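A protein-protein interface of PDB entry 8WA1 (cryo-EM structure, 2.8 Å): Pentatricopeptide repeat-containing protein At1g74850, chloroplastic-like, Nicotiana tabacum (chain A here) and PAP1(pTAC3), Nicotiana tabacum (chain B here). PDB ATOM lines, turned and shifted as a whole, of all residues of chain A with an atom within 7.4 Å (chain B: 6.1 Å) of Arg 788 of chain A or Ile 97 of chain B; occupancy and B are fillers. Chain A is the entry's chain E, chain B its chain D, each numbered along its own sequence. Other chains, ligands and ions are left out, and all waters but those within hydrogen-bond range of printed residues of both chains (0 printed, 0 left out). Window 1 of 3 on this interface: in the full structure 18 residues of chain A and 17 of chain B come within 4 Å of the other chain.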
ATOM      1  N   GLU A 469      20.091  10.172 -40.099  1.00  0.00           N
ATOM      2  CA  GLU A 469      18.666  10.358 -40.358  1.00  0.00           C
ATOM      3  C   GLU A 469      18.435  11.347 -41.494  1.00  0.00           C
ATOM      4  O   GLU A 469      17.534  11.157 -42.321  1.00  0.00           O
ATOM      5  CB  GLU A 469      17.956  10.823 -39.088  1.00  0.00           C
ATOM      6  CG  GLU A 469      17.920   9.785 -37.977  1.00  0.00           C
ATOM      7  CD  GLU A 469      16.971   8.638 -38.275  1.00  0.00           C
ATOM      8  OE1 GLU A 469      16.088   8.802 -39.143  1.00  0.00           O
ATOM      9  OE2 GLU A 469      17.109   7.572 -37.639  1.00  0.00           O
ATOM     10  N   SER A 707      28.239  15.098 -23.756  1.00  0.00           N
ATOM     11  CA  SER A 707      28.591  13.769 -24.229  1.00  0.00           C
ATOM     12  C   SER A 707      29.722  13.846 -25.245  1.00  0.00           C
ATOM     13  O   SER A 707      29.958  14.883 -25.871  1.00  0.00           O
ATOM     14  CB  SER A 707      27.383  13.056 -24.851  1.00  0.00           C
ATOM     15  OG  SER A 707      27.765  11.817 -25.424  1.00  0.00           O
ATOM     16  N   VAL A 708      30.419  12.722 -25.398  1.00  0.00           N
ATOM     17  CA  VAL A 708      31.483  12.565 -26.381  1.00  0.00           C
ATOM     18  C   VAL A 708      31.122  11.386 -27.276  1.00  0.00           C
ATOM     19  O   VAL A 708      30.901  10.271 -26.788  1.00  0.00           O
ATOM     20  CB  VAL A 708      32.857  12.362 -25.719  1.00  0.00           C
ATOM     21  CG1 VAL A 708      32.760  11.387 -24.551  1.00  0.00           C
ATOM     22  CG2 VAL A 708      33.875  11.879 -26.743  1.00  0.00           C
ATOM     23  N   ASP A 709      31.052  11.634 -28.581  1.00  0.00           N
ATOM     24  CA  ASP A 709      30.670  10.621 -29.556  1.00  0.00           C
ATOM     25  C   ASP A 709      31.924   9.971 -30.125  1.00  0.00           C
ATOM     26  O   ASP A 709      32.762  10.649 -30.728  1.00  0.00           O
ATOM     27  CB  ASP A 709      29.828  11.231 -30.675  1.00  0.00           C
ATOM     28  CG  ASP A 709      29.699  10.310 -31.873  1.00  0.00           C
ATOM     29  OD1 ASP A 709      28.965   9.303 -31.778  1.00  0.00           O
ATOM     30  OD2 ASP A 709      30.334  10.591 -32.909  1.00  0.00           O
ATOM     31  N   LEU A 742      23.031  14.185 -17.441  1.00  0.00           N
ATOM     32  CA  LEU A 742      23.574  12.896 -17.848  1.00  0.00           C
ATOM     33  C   LEU A 742      24.851  13.121 -18.644  1.00  0.00           C
ATOM     34  O   LEU A 742      24.833  13.811 -19.667  1.00  0.00           O
ATOM     35  CB  LEU A 742      22.562  12.106 -18.683  1.00  0.00           C
ATOM     36  CG  LEU A 742      22.870  10.621 -18.881  1.00  0.00           C
ATOM     37  CD1 LEU A 742      22.762   9.878 -17.558  1.00  0.00           C
ATOM     38  CD2 LEU A 742      21.947  10.009 -19.925  1.00  0.00           C
ATOM     39  N   SER A 744      27.389  11.268 -20.910  1.00  0.00           N
ATOM     40  CA  SER A 744      27.360  10.051 -21.706  1.00  0.00           C
ATOM     41  C   SER A 744      28.584   9.977 -22.606  1.00  0.00           C
ATOM     42  O   SER A 744      29.216  10.987 -22.922  1.00  0.00           O
ATOM     43  CB  SER A 744      26.085   9.969 -22.555  1.00  0.00           C
ATOM     44  OG  SER A 744      26.081   8.803 -23.360  1.00  0.00           O
ATOM     45  N   VAL A 745      28.912   8.754 -23.014  1.00  0.00           N
ATOM     46  CA  VAL A 745      29.993   8.486 -23.958  1.00  0.00           C
ATOM     47  C   VAL A 745      29.413   7.613 -25.063  1.00  0.00           C
ATOM     48  O   VAL A 745      29.238   6.402 -24.877  1.00  0.00           O
ATOM     49  CB  VAL A 745      31.194   7.805 -23.287  1.00  0.00           C
ATOM     50  CG1 VAL A 745      32.300   7.555 -24.302  1.00  0.00           C
ATOM     51  CG2 VAL A 745      31.710   8.648 -22.130  1.00  0.00           C
ATOM     52  N   VAL A 746      29.114   8.224 -26.209  1.00  0.00           N
ATOM     53  CA  VAL A 746      28.510   7.489 -27.313  1.00  0.00           C
ATOM     54  C   VAL A 746      29.538   6.549 -27.928  1.00  0.00           C
ATOM     55  O   VAL A 746      30.668   6.950 -28.240  1.00  0.00           O
ATOM     56  CB  VAL A 746      27.946   8.460 -28.363  1.00  0.00           C
ATOM     57  CG1 VAL A 746      27.210   7.695 -29.454  1.00  0.00           C
ATOM     58  CG2 VAL A 746      27.030   9.481 -27.705  1.00  0.00           C
ATOM     59  N   VAL A 747      29.149   5.287 -28.103  1.00  0.00           N
ATOM     60  CA  VAL A 747      30.008   4.263 -28.685  1.00  0.00           C
ATOM     61  C   VAL A 747      29.412   3.691 -29.967  1.00  0.00           C
ATOM     62  O   VAL A 747      30.092   3.602 -30.994  1.00  0.00           O
ATOM     63  CB  VAL A 747      30.308   3.134 -27.669  1.00  0.00           C
ATOM     64  CG1 VAL A 747      29.091   2.839 -26.815  1.00  0.00           C
ATOM     65  CG2 VAL A 747      30.759   1.880 -28.392  1.00  0.00           C
ATOM     66  N   VAL A 748      28.138   3.310 -29.931  1.00  0.00           N
ATOM     67  CA  VAL A 748      27.459   2.726 -31.082  1.00  0.00           C
ATOM     68  C   VAL A 748      26.117   3.425 -31.252  1.00  0.00           C
ATOM     69  O   VAL A 748      25.287   3.429 -30.333  1.00  0.00           O
ATOM     70  CB  VAL A 748      27.283   1.204 -30.936  1.00  0.00           C
ATOM     71  CG1 VAL A 748      27.028   0.828 -29.485  1.00  0.00           C
ATOM     72  CG2 VAL A 748      26.157   0.704 -31.832  1.00  0.00           C
ATOM     73  N   ARG A 749      25.909   4.025 -32.423  1.00  0.00           N
ATOM     74  CA  ARG A 749      24.673   4.717 -32.783  1.00  0.00           C
ATOM     75  C   ARG A 749      24.158   4.094 -34.077  1.00  0.00           C
ATOM     76  O   ARG A 749      24.580   4.471 -35.172  1.00  0.00           O
ATOM     77  CB  ARG A 749      24.903   6.225 -32.934  1.00  0.00           C
ATOM     78  CG  ARG A 749      23.674   7.001 -33.390  1.00  0.00           C
ATOM     79  CD  ARG A 749      24.015   8.449 -33.721  1.00  0.00           C
ATOM     80  NE  ARG A 749      22.865   9.166 -34.269  1.00  0.00           N
ATOM     81  CZ  ARG A 749      22.901  10.424 -34.696  1.00  0.00           C
ATOM     82  NH1 ARG A 749      21.805  10.994 -35.178  1.00  0.00           N
ATOM     83  NH2 ARG A 749      24.033  11.114 -34.643  1.00  0.00           N
ATOM     84  N   GLY A 750      23.245   3.135 -33.948  1.00  0.00           N
ATOM     85  CA  GLY A 750      22.712   2.449 -35.112  1.00  0.00           C
ATOM     86  C   GLY A 750      21.421   1.737 -34.781  1.00  0.00           C
ATOM     87  O   GLY A 750      20.817   1.944 -33.726  1.00  0.00           O
ATOM     88  N   GLU A 753      21.483  -0.791 -31.596  1.00  0.00           N
ATOM     89  CA  GLU A 753      21.690  -0.309 -30.234  1.00  0.00           C
ATOM     90  C   GLU A 753      20.855  -1.103 -29.235  1.00  0.00           C
ATOM     91  O   GLU A 753      21.346  -1.483 -28.166  1.00  0.00           O
ATOM     92  CB  GLU A 753      21.362   1.180 -30.141  1.00  0.00           C
ATOM     93  CG  GLU A 753      22.268   2.070 -30.970  1.00  0.00           C
ATOM     94  CD  GLU A 753      21.966   3.542 -30.778  1.00  0.00           C
ATOM     95  OE1 GLU A 753      22.063   4.022 -29.629  1.00  0.00           O
ATOM     96  OE2 GLU A 753      21.622   4.214 -31.771  1.00  0.00           O
ATOM     97  N   THR A 758      26.622  -5.501 -27.615  1.00  0.00           N
ATOM     98  CA  THR A 758      27.484  -4.403 -27.186  1.00  0.00           C
ATOM     99  C   THR A 758      28.916  -4.873 -26.962  1.00  0.00           C
ATOM    100  O   THR A 758      29.868  -4.119 -27.189  1.00  0.00           O
ATOM    101  CB  THR A 758      26.926  -3.767 -25.912  1.00  0.00           C
ATOM    102  OG1 THR A 758      27.077  -4.675 -24.815  1.00  0.00           O
ATOM    103  CG2 THR A 758      25.450  -3.447 -26.088  1.00  0.00           C
ATOM    104  N   CYS A 780      28.387   3.122 -16.586  1.00  0.00           N
ATOM    105  CA  CYS A 780      27.805   1.834 -16.930  1.00  0.00           C
ATOM    106  C   CYS A 780      26.795   2.008 -18.056  1.00  0.00           C
ATOM    107  O   CYS A 780      26.261   3.099 -18.272  1.00  0.00           O
ATOM    108  CB  CYS A 780      27.129   1.180 -15.716  1.00  0.00           C
ATOM    109  SG  CYS A 780      25.776   2.145 -15.009  1.00  0.00           S
ATOM    110  N   PHE A 781      26.547   0.917 -18.774  1.00  0.00           N
ATOM    111  CA  PHE A 781      25.559   0.940 -19.840  1.00  0.00           C
ATOM    112  C   PHE A 781      24.164   1.131 -19.250  1.00  0.00           C
ATOM    113  O   PHE A 781      23.733   0.339 -18.402  1.00  0.00           O
ATOM    114  CB  PHE A 781      25.616  -0.353 -20.656  1.00  0.00           C
ATOM    115  CG  PHE A 781      26.911  -0.547 -21.395  1.00  0.00           C
ATOM    116  CD1 PHE A 781      27.987  -1.174 -20.787  1.00  0.00           C
ATOM    117  CD2 PHE A 781      27.052  -0.102 -22.700  1.00  0.00           C
ATOM    118  CE1 PHE A 781      29.178  -1.351 -21.465  1.00  0.00           C
ATOM    119  CE2 PHE A 781      28.242  -0.277 -23.383  1.00  0.00           C
ATOM    120  CZ  PHE A 781      29.306  -0.902 -22.765  1.00  0.00           C
ATOM    121  N   PRO A 782      23.431   2.164 -19.668  1.00  0.00           N
ATOM    122  CA  PRO A 782      22.138   2.455 -19.039  1.00  0.00           C
ATOM    123  C   PRO A 782      20.990   1.632 -19.599  1.00  0.00           C
ATOM    124  O   PRO A 782      21.142   0.922 -20.599  1.00  0.00           O
ATOM    125  CB  PRO A 782      21.947   3.945 -19.330  1.00  0.00           C
ATOM    126  CG  PRO A 782      22.633   4.142 -20.635  1.00  0.00           C
ATOM    127  CD  PRO A 782      23.812   3.196 -20.648  1.00  0.00           C
ATOM    128  N   TRP A 784      17.879   2.919 -20.601  1.00  0.00           N
ATOM    129  CA  TRP A 784      17.135   3.587 -21.667  1.00  0.00           C
ATOM    130  C   TRP A 784      17.761   3.318 -23.030  1.00  0.00           C
ATOM    131  O   TRP A 784      17.059   3.255 -24.047  1.00  0.00           O
ATOM    132  CB  TRP A 784      17.044   5.091 -21.392  1.00  0.00           C
ATOM    133  CG  TRP A 784      18.316   5.724 -20.915  1.00  0.00           C
ATOM    134  CD1 TRP A 784      19.358   6.156 -21.683  1.00  0.00           C
ATOM    135  CD2 TRP A 784      18.669   6.019 -19.558  1.00  0.00           C
ATOM    136  NE1 TRP A 784      20.342   6.694 -20.887  1.00  0.00           N
ATOM    137  CE2 TRP A 784      19.942   6.623 -19.579  1.00  0.00           C
ATOM    138  CE3 TRP A 784      18.034   5.829 -18.327  1.00  0.00           C
ATOM    139  CZ2 TRP A 784      20.593   7.033 -18.418  1.00  0.00           C
ATOM    140  CZ3 TRP A 784      18.682   6.239 -17.175  1.00  0.00           C
ATOM    141  CH2 TRP A 784      19.948   6.833 -17.230  1.00  0.00           C
ATOM    142  N   ASN A 785      19.080   3.148 -23.071  1.00  0.00           N
ATOM    143  CA  ASN A 785      19.756   2.762 -24.302  1.00  0.00           C
ATOM    144  C   ASN A 785      20.995   1.954 -23.947  1.00  0.00           C
ATOM    145  O   ASN A 785      21.726   2.288 -23.013  1.00  0.00           O
ATOM    146  CB  ASN A 785      20.141   3.980 -25.149  1.00  0.00           C
ATOM    147  CG  ASN A 785      20.437   3.618 -26.594  1.00  0.00           C
ATOM    148  OD1 ASN A 785      20.897   2.515 -26.892  1.00  0.00           O
ATOM    149  ND2 ASN A 785      20.169   4.550 -27.501  1.00  0.00           N
ATOM    150  N   LYS A 786      21.218   0.884 -24.704  1.00  0.00           N
ATOM    151  CA  LYS A 786      22.374   0.020 -24.510  1.00  0.00           C
ATOM    152  C   LYS A 786      23.514   0.329 -25.471  1.00  0.00           C
ATOM    153  O   LYS A 786      24.468  -0.451 -25.547  1.00  0.00           O
ATOM    154  CB  LYS A 786      21.962  -1.450 -24.652  1.00  0.00           C
ATOM    155  CG  LYS A 786      20.966  -1.914 -23.601  1.00  0.00           C
ATOM    156  CD  LYS A 786      20.451  -3.313 -23.899  1.00  0.00           C
ATOM    157  CE  LYS A 786      19.665  -3.342 -25.200  1.00  0.00           C
ATOM    158  NZ  LYS A 786      19.096  -4.689 -25.477  1.00  0.00           N
ATOM    159  N   GLY A 787      23.440   1.439 -26.201  1.00  0.00           N
ATOM    160  CA  GLY A 787      24.459   1.765 -27.179  1.00  0.00           C
ATOM    161  C   GLY A 787      25.390   2.882 -26.758  1.00  0.00           C
ATOM    162  O   GLY A 787      26.097   3.451 -27.595  1.00  0.00           O
ATOM    163  N   ARG A 788      25.386   3.219 -25.471  1.00  0.00           N
ATOM    164  CA  ARG A 788      26.274   4.228 -24.920  1.00  0.00           C
ATOM    165  C   ARG A 788      26.620   3.892 -23.474  1.00  0.00           C
ATOM    166  O   ARG A 788      26.110   2.928 -22.897  1.00  0.00           O
ATOM    167  CB  ARG A 788      25.653   5.630 -25.002  1.00  0.00           C
ATOM    168  CG  ARG A 788      24.148   5.679 -24.787  1.00  0.00           C
ATOM    169  CD  ARG A 788      23.400   5.682 -26.116  1.00  0.00           C
ATOM    170  NE  ARG A 788      23.814   6.790 -26.969  1.00  0.00           N
ATOM    171  CZ  ARG A 788      23.343   7.012 -28.191  1.00  0.00           C
ATOM    172  NH1 ARG A 788      22.434   6.201 -28.712  1.00  0.00           N
ATOM    173  NH2 ARG A 788      23.779   8.048 -28.895  1.00  0.00           N
ATOM    174  N   ILE A 789      27.502   4.704 -22.895  1.00  0.00           N
ATOM    175  CA  ILE A 789      27.877   4.610 -21.489  1.00  0.00           C
ATOM    176  C   ILE A 789      27.665   5.979 -20.862  1.00  0.00           C
ATOM    177  O   ILE A 789      28.164   6.984 -21.381  1.00  0.00           O
ATOM    178  CB  ILE A 789      29.336   4.153 -21.307  1.00  0.00           C
ATOM    179  CG1 ILE A 789      29.569   2.809 -21.999  1.00  0.00           C
ATOM    180  CG2 ILE A 789      29.680   4.055 -19.831  1.00  0.00           C
ATOM    181  CD1 ILE A 789      30.988   2.300 -21.878  1.00  0.00           C
ATOM    182  N   VAL A 790      26.926   6.023 -19.753  1.00  0.00           N
ATOM    183  CA  VAL A 790      26.485   7.282 -19.166  1.00  0.00           C
ATOM    184  C   VAL A 790      26.893   7.349 -17.700  1.00  0.00           C
ATOM    185  O   VAL A 790      27.256   6.342 -17.087  1.00  0.00           O
ATOM    186  CB  VAL A 790      24.959   7.476 -19.294  1.00  0.00           C
ATOM    187  CG1 VAL A 790      24.509   7.283 -20.732  1.00  0.00           C
ATOM    188  CG2 VAL A 790      24.228   6.528 -18.360  1.00  0.00           C
ATOM    189  N   VAL B  92      18.152  19.997 -29.189  1.00  0.00           N
ATOM    190  CA  VAL B  92      17.610  19.168 -28.114  1.00  0.00           C
ATOM    191  C   VAL B  92      17.341  17.752 -28.611  1.00  0.00           C
ATOM    192  O   VAL B  92      17.564  16.773 -27.889  1.00  0.00           O
ATOM    193  CB  VAL B  92      16.342  19.818 -27.526  1.00  0.00           C
ATOM    194  CG1 VAL B  92      15.641  18.865 -26.569  1.00  0.00           C
ATOM    195  CG2 VAL B  92      16.695  21.114 -26.813  1.00  0.00           C
ATOM    196  N   ILE B  93      16.866  17.619 -29.851  1.00  0.00           N
ATOM    197  CA  ILE B  93      16.627  16.289 -30.408  1.00  0.00           C
ATOM    198  C   ILE B  93      17.935  15.518 -30.535  1.00  0.00           C
ATOM    199  O   ILE B  93      18.017  14.338 -30.163  1.00  0.00           O
ATOM    200  CB  ILE B  93      15.896  16.397 -31.760  1.00  0.00           C
ATOM    201  CG1 ILE B  93      14.473  16.921 -31.558  1.00  0.00           C
ATOM    202  CG2 ILE B  93      15.869  15.048 -32.463  1.00  0.00           C
ATOM    203  CD1 ILE B  93      13.702  17.109 -32.848  1.00  0.00           C
ATOM    204  N   TYR B  94      18.984  16.168 -31.046  1.00  0.00           N
ATOM    205  CA  TYR B  94      20.277  15.496 -31.148  1.00  0.00           C
ATOM    206  C   TYR B  94      20.862  15.208 -29.770  1.00  0.00           C
ATOM    207  O   TYR B  94      21.578  14.218 -29.588  1.00  0.00           O
ATOM    208  CB  TYR B  94      21.244  16.330 -31.987  1.00  0.00           C
ATOM    209  CG  TYR B  94      21.108  16.088 -33.472  1.00  0.00           C
ATOM    210  CD1 TYR B  94      20.638  14.874 -33.954  1.00  0.00           C
ATOM    211  CD2 TYR B  94      21.445  17.072 -34.392  1.00  0.00           C
ATOM    212  CE1 TYR B  94      20.509  14.644 -35.311  1.00  0.00           C
ATOM    213  CE2 TYR B  94      21.319  16.852 -35.751  1.00  0.00           C
ATOM    214  CZ  TYR B  94      20.851  15.636 -36.204  1.00  0.00           C
ATOM    215  OH  TYR B  94      20.723  15.409 -37.556  1.00  0.00           O
ATOM    216  N   ASP B  95      20.555  16.050 -28.782  1.00  0.00           N
ATOM    217  CA  ASP B  95      20.995  15.781 -27.417  1.00  0.00           C
ATOM    218  C   ASP B  95      20.312  14.543 -26.855  1.00  0.00           C
ATOM    219  O   ASP B  95      20.945  13.731 -26.171  1.00  0.00           O
ATOM    220  CB  ASP B  95      20.722  16.996 -26.532  1.00  0.00           C
ATOM    221  CG  ASP B  95      21.642  18.158 -26.842  1.00  0.00           C
ATOM    222  OD1 ASP B  95      22.487  18.021 -27.751  1.00  0.00           O
ATOM    223  OD2 ASP B  95      21.521  19.210 -26.179  1.00  0.00           O
ATOM    224  N   MET B  96      19.014  14.386 -27.128  1.00  0.00           N
ATOM    225  CA  MET B  96      18.320  13.162 -26.733  1.00  0.00           C
ATOM    226  C   MET B  96      18.912  11.950 -27.437  1.00  0.00           C
ATOM    227  O   MET B  96      19.067  10.883 -26.832  1.00  0.00           O
ATOM    228  CB  MET B  96      16.826  13.270 -27.041  1.00  0.00           C
ATOM    229  CG  MET B  96      16.118  14.434 -26.379  1.00  0.00           C
ATOM    230  SD  MET B  96      14.326  14.253 -26.426  1.00  0.00           S
ATOM    231  CE  MET B  96      14.087  13.778 -28.134  1.00  0.00           C
ATOM    232  N   ILE B  97      19.236  12.094 -28.725  1.00  0.00           N
ATOM    233  CA  ILE B  97      19.816  10.984 -29.478  1.00  0.00           C
ATOM    234  C   ILE B  97      21.166  10.584 -28.893  1.00  0.00           C
ATOM    235  O   ILE B  97      21.472   9.392 -28.757  1.00  0.00           O
ATOM    236  CB  ILE B  97      19.928  11.354 -30.970  1.00  0.00           C
ATOM    237  CG1 ILE B  97      18.535  11.496 -31.586  1.00  0.00           C
ATOM    238  CG2 ILE B  97      20.745  10.316 -31.722  1.00  0.00           C
ATOM    239  CD1 ILE B  97      18.548  11.888 -33.046  1.00  0.00           C
ATOM    240  N   ALA B  98      21.989  11.571 -28.528  1.00  0.00           N
ATOM    241  CA  ALA B  98      23.308  11.272 -27.979  1.00  0.00           C
ATOM    242  C   ALA B  98      23.208  10.683 -26.578  1.00  0.00           C
ATOM    243  O   ALA B  98      23.926   9.733 -26.242  1.00  0.00           O
ATOM    244  CB  ALA B  98      24.168  12.535 -27.969  1.00  0.00           C
ATOM    245  N   ALA B  99      22.321  11.231 -25.745  1.00  0.00           N
ATOM    246  CA  ALA B  99      22.158  10.748 -24.380  1.00  0.00           C
ATOM    247  C   ALA B  99      21.451   9.403 -24.307  1.00  0.00           C
ATOM    248  O   ALA B  99      21.326   8.848 -23.209  1.00  0.00           O
ATOM    249  CB  ALA B  99      21.395  11.779 -23.546  1.00  0.00           C
ATOM    250  N   GLY B 100      20.981   8.872 -25.434  1.00  0.00           N
ATOM    251  CA  GLY B 100      20.324   7.586 -25.465  1.00  0.00           C
ATOM    252  C   GLY B 100      18.815   7.628 -25.364  1.00  0.00           C
ATOM    253  O   GLY B 100      18.171   6.587 -25.549  1.00  0.00           O
ATOM    254  N   LEU B 101      18.228   8.787 -25.081  1.00  0.00           N
ATOM    255  CA  LEU B 101      16.776   8.914 -25.002  1.00  0.00           C
ATOM    256  C   LEU B 101      16.218   8.974 -26.418  1.00  0.00           C
ATOM    257  O   LEU B 101      16.298  10.014 -27.082  1.00  0.00           O
ATOM    258  CB  LEU B 101      16.391  10.155 -24.203  1.00  0.00           C
ATOM    259  CG  LEU B 101      16.958  10.261 -22.786  1.00  0.00           C
ATOM    260  CD1 LEU B 101      16.572  11.589 -22.151  1.00  0.00           C
ATOM    261  CD2 LEU B 101      16.489   9.098 -21.925  1.00  0.00           C
ATOM    262  N   SER B 102      15.656   7.862 -26.885  1.00  0.00           N
ATOM    263  CA  SER B 102      15.132   7.806 -28.238  1.00  0.00           C
ATOM    264  C   SER B 102      13.946   8.759 -28.389  1.00  0.00           C
ATOM    265  O   SER B 102      13.086   8.838 -27.509  1.00  0.00           O
ATOM    266  CB  SER B 102      14.703   6.384 -28.588  1.00  0.00           C
ATOM    267  OG  SER B 102      14.223   6.309 -29.919  1.00  0.00           O
ATOM    268  N   PRO B 103      13.882   9.494 -29.497  1.00  0.00           N
ATOM    269  CA  PRO B 103      12.779  10.438 -29.694  1.00  0.00           C
ATOM    270  C   PRO B 103      11.446   9.723 -29.845  1.00  0.00           C
ATOM    271  O   PRO B 103      11.372   8.513 -30.071  1.00  0.00           O
ATOM    272  CB  PRO B 103      13.163  11.174 -30.983  1.00  0.00           C
ATOM    273  CG  PRO B 103      14.638  10.956 -31.127  1.00  0.00           C
ATOM    274  CD  PRO B 103      14.891   9.592 -30.565  1.00  0.00           C
ATOM    275  N   ARG B 130      11.139  13.053 -41.340  1.00  0.00           N
ATOM    276  CA  ARG B 130      12.072  12.453 -40.393  1.00  0.00           C
ATOM    277  C   ARG B 130      11.334  11.617 -39.354  1.00  0.00           C
ATOM    278  O   ARG B 130      11.754  10.500 -39.026  1.00  0.00           O
ATOM    279  CB  ARG B 130      12.910  13.539 -39.716  1.00  0.00           C
ATOM    280  CG  ARG B 130      13.894  14.237 -40.643  1.00  0.00           C
ATOM    281  CD  ARG B 130      15.335  14.043 -40.191  1.00  0.00           C
ATOM    282  NE  ARG B 130      15.610  14.678 -38.905  1.00  0.00           N
ATOM    283  CZ  ARG B 130      15.650  14.032 -37.743  1.00  0.00           C
ATOM    284  NH1 ARG B 130      15.434  12.725 -37.701  1.00  0.00           N
ATOM    285  NH2 ARG B 130      15.909  14.693 -36.622  1.00  0.00           N
ATOM    286  N   GLU B 134      11.519   7.593 -38.850  1.00  0.00           N
ATOM    287  CA  GLU B 134      11.841   7.047 -37.538  1.00  0.00           C
ATOM    288  C   GLU B 134      10.993   5.836 -37.172  1.00  0.00           C
ATOM    289  O   GLU B 134      11.324   5.144 -36.202  1.00  0.00           O
ATOM    290  CB  GLU B 134      11.681   8.132 -36.470  1.00  0.00           C
ATOM    291  CG  GLU B 134      12.855   8.248 -35.513  1.00  0.00           C
ATOM    292  CD  GLU B 134      14.093   8.835 -36.167  1.00  0.00           C
ATOM    293  OE1 GLU B 134      13.985   9.361 -37.296  1.00  0.00           O
ATOM    294  OE2 GLU B 134      15.177   8.773 -35.549  1.00  0.00           O
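NE of Arg 788 of chain A is in hydrogen-bond range of O of Ala 98 of chain B, at 3.0 Å. The side-chain carboxylate (OE1) of Glu 134 of chain B lies close to the side-chain carboxylate (OE1) of Glu 469 of chain A. The backbone carbonyl oxygen (O) of Ile 97 of chain B sits at hydrogen-bond distance from the guanidinium group (NH2) of Arg 788 of chain A, 2.7 Å away. The backbone carbonyl oxygen (O) of Gly 100 of chain B sits close to the side-chain amide nitrogen (ND2) of Asn 785 of chain A (3.5 Å). NE1 of Trp 784 of chain A is in hydrogen-bond range of O of Ala 99 of chain B (3.3 Å).
The side-chain carboxylate (OE2) of Glu 753 of chain A is in salt-bridge range of the guanidinium group (NH1) of Arg 788 of chain A, at 3.7 Å. The side-chain amide nitrogen of Asn 785 of chain A sits at hydrogen-bond distance from the side-chain carboxylate of Glu 753 of chain A. The backbone carbonyl oxygen of Ser 744 of chain A lies within hydrogen-bond range of the side-chain hydroxyl of Ser 707 of chain A (3.0 Å). O of Met 96 of chain B is in hydrogen-bond range of N of Leu 101 of chain B (2.9 Å). NH1 of Arg 130 of chain B is in salt-bridge range of OE1 of Glu 134 of chain B, 3.7 Å away. NH1 of Arg 788 of chain A lies close to ND2 of Asn 785 of chain A (3.1 Å).
Among the printed residues, pairs that only touch across the chains: Glu 469 of chain A with Arg 130 of chain B, Leu 742 of chain A with Ala 99 of chain B, Ser 744 of chain A with Ala 98 of chain B, Val 746 of chain A with Ala 98 of chain B, Arg 749 of chain A with Tyr 94 of chain B, Arg 749 of chain A with Ile 97 of chain B, Trp 784 of chain A with Gly 100 of chain B, Trp 784 of chain A with Leu 101 of chain B and Arg 788 of chain A with Gly 100 of chain B.
Printed residues of chain B within 4 Å of Glu 469 of chain A: Arg 130 and Glu 134. Of chain B, only Ile 97, Ala 98 and Gly 100 come within 4 Å of Arg 788 of chain A. Ile 97 of chain B touches just these residues of chain A: Arg 749 and Arg 788. Printed residues of chain A within 4 Å of Gly 100 of chain B: Trp 784 (3.8 Å), Asn 785 (3.3 Å) and Arg 788 (3.7 Å).
Of the 14 printed residues of chain B, 8 touch a printed residue of chain A. Hydrophobic or aromatic side chains of chain B that line the printed part of chain A: Tyr 94, Ile 97 and Leu 101. Of the 24 printed residues of chain A, 8 touch a printed residue of chain B. Printed residues of chain A that touch a printed residue of chain B: Glu 469, Leu 742, Ser 744, Val 746, Arg 749, Trp 784, Asn 785 and Arg 788. Hydrophobic or aromatic side chains of chain A within 4 Å of the printed part of chain B: Leu 742, Val 746 and Trp 784. Among the printed residues, 14 pairs touch across the chains.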
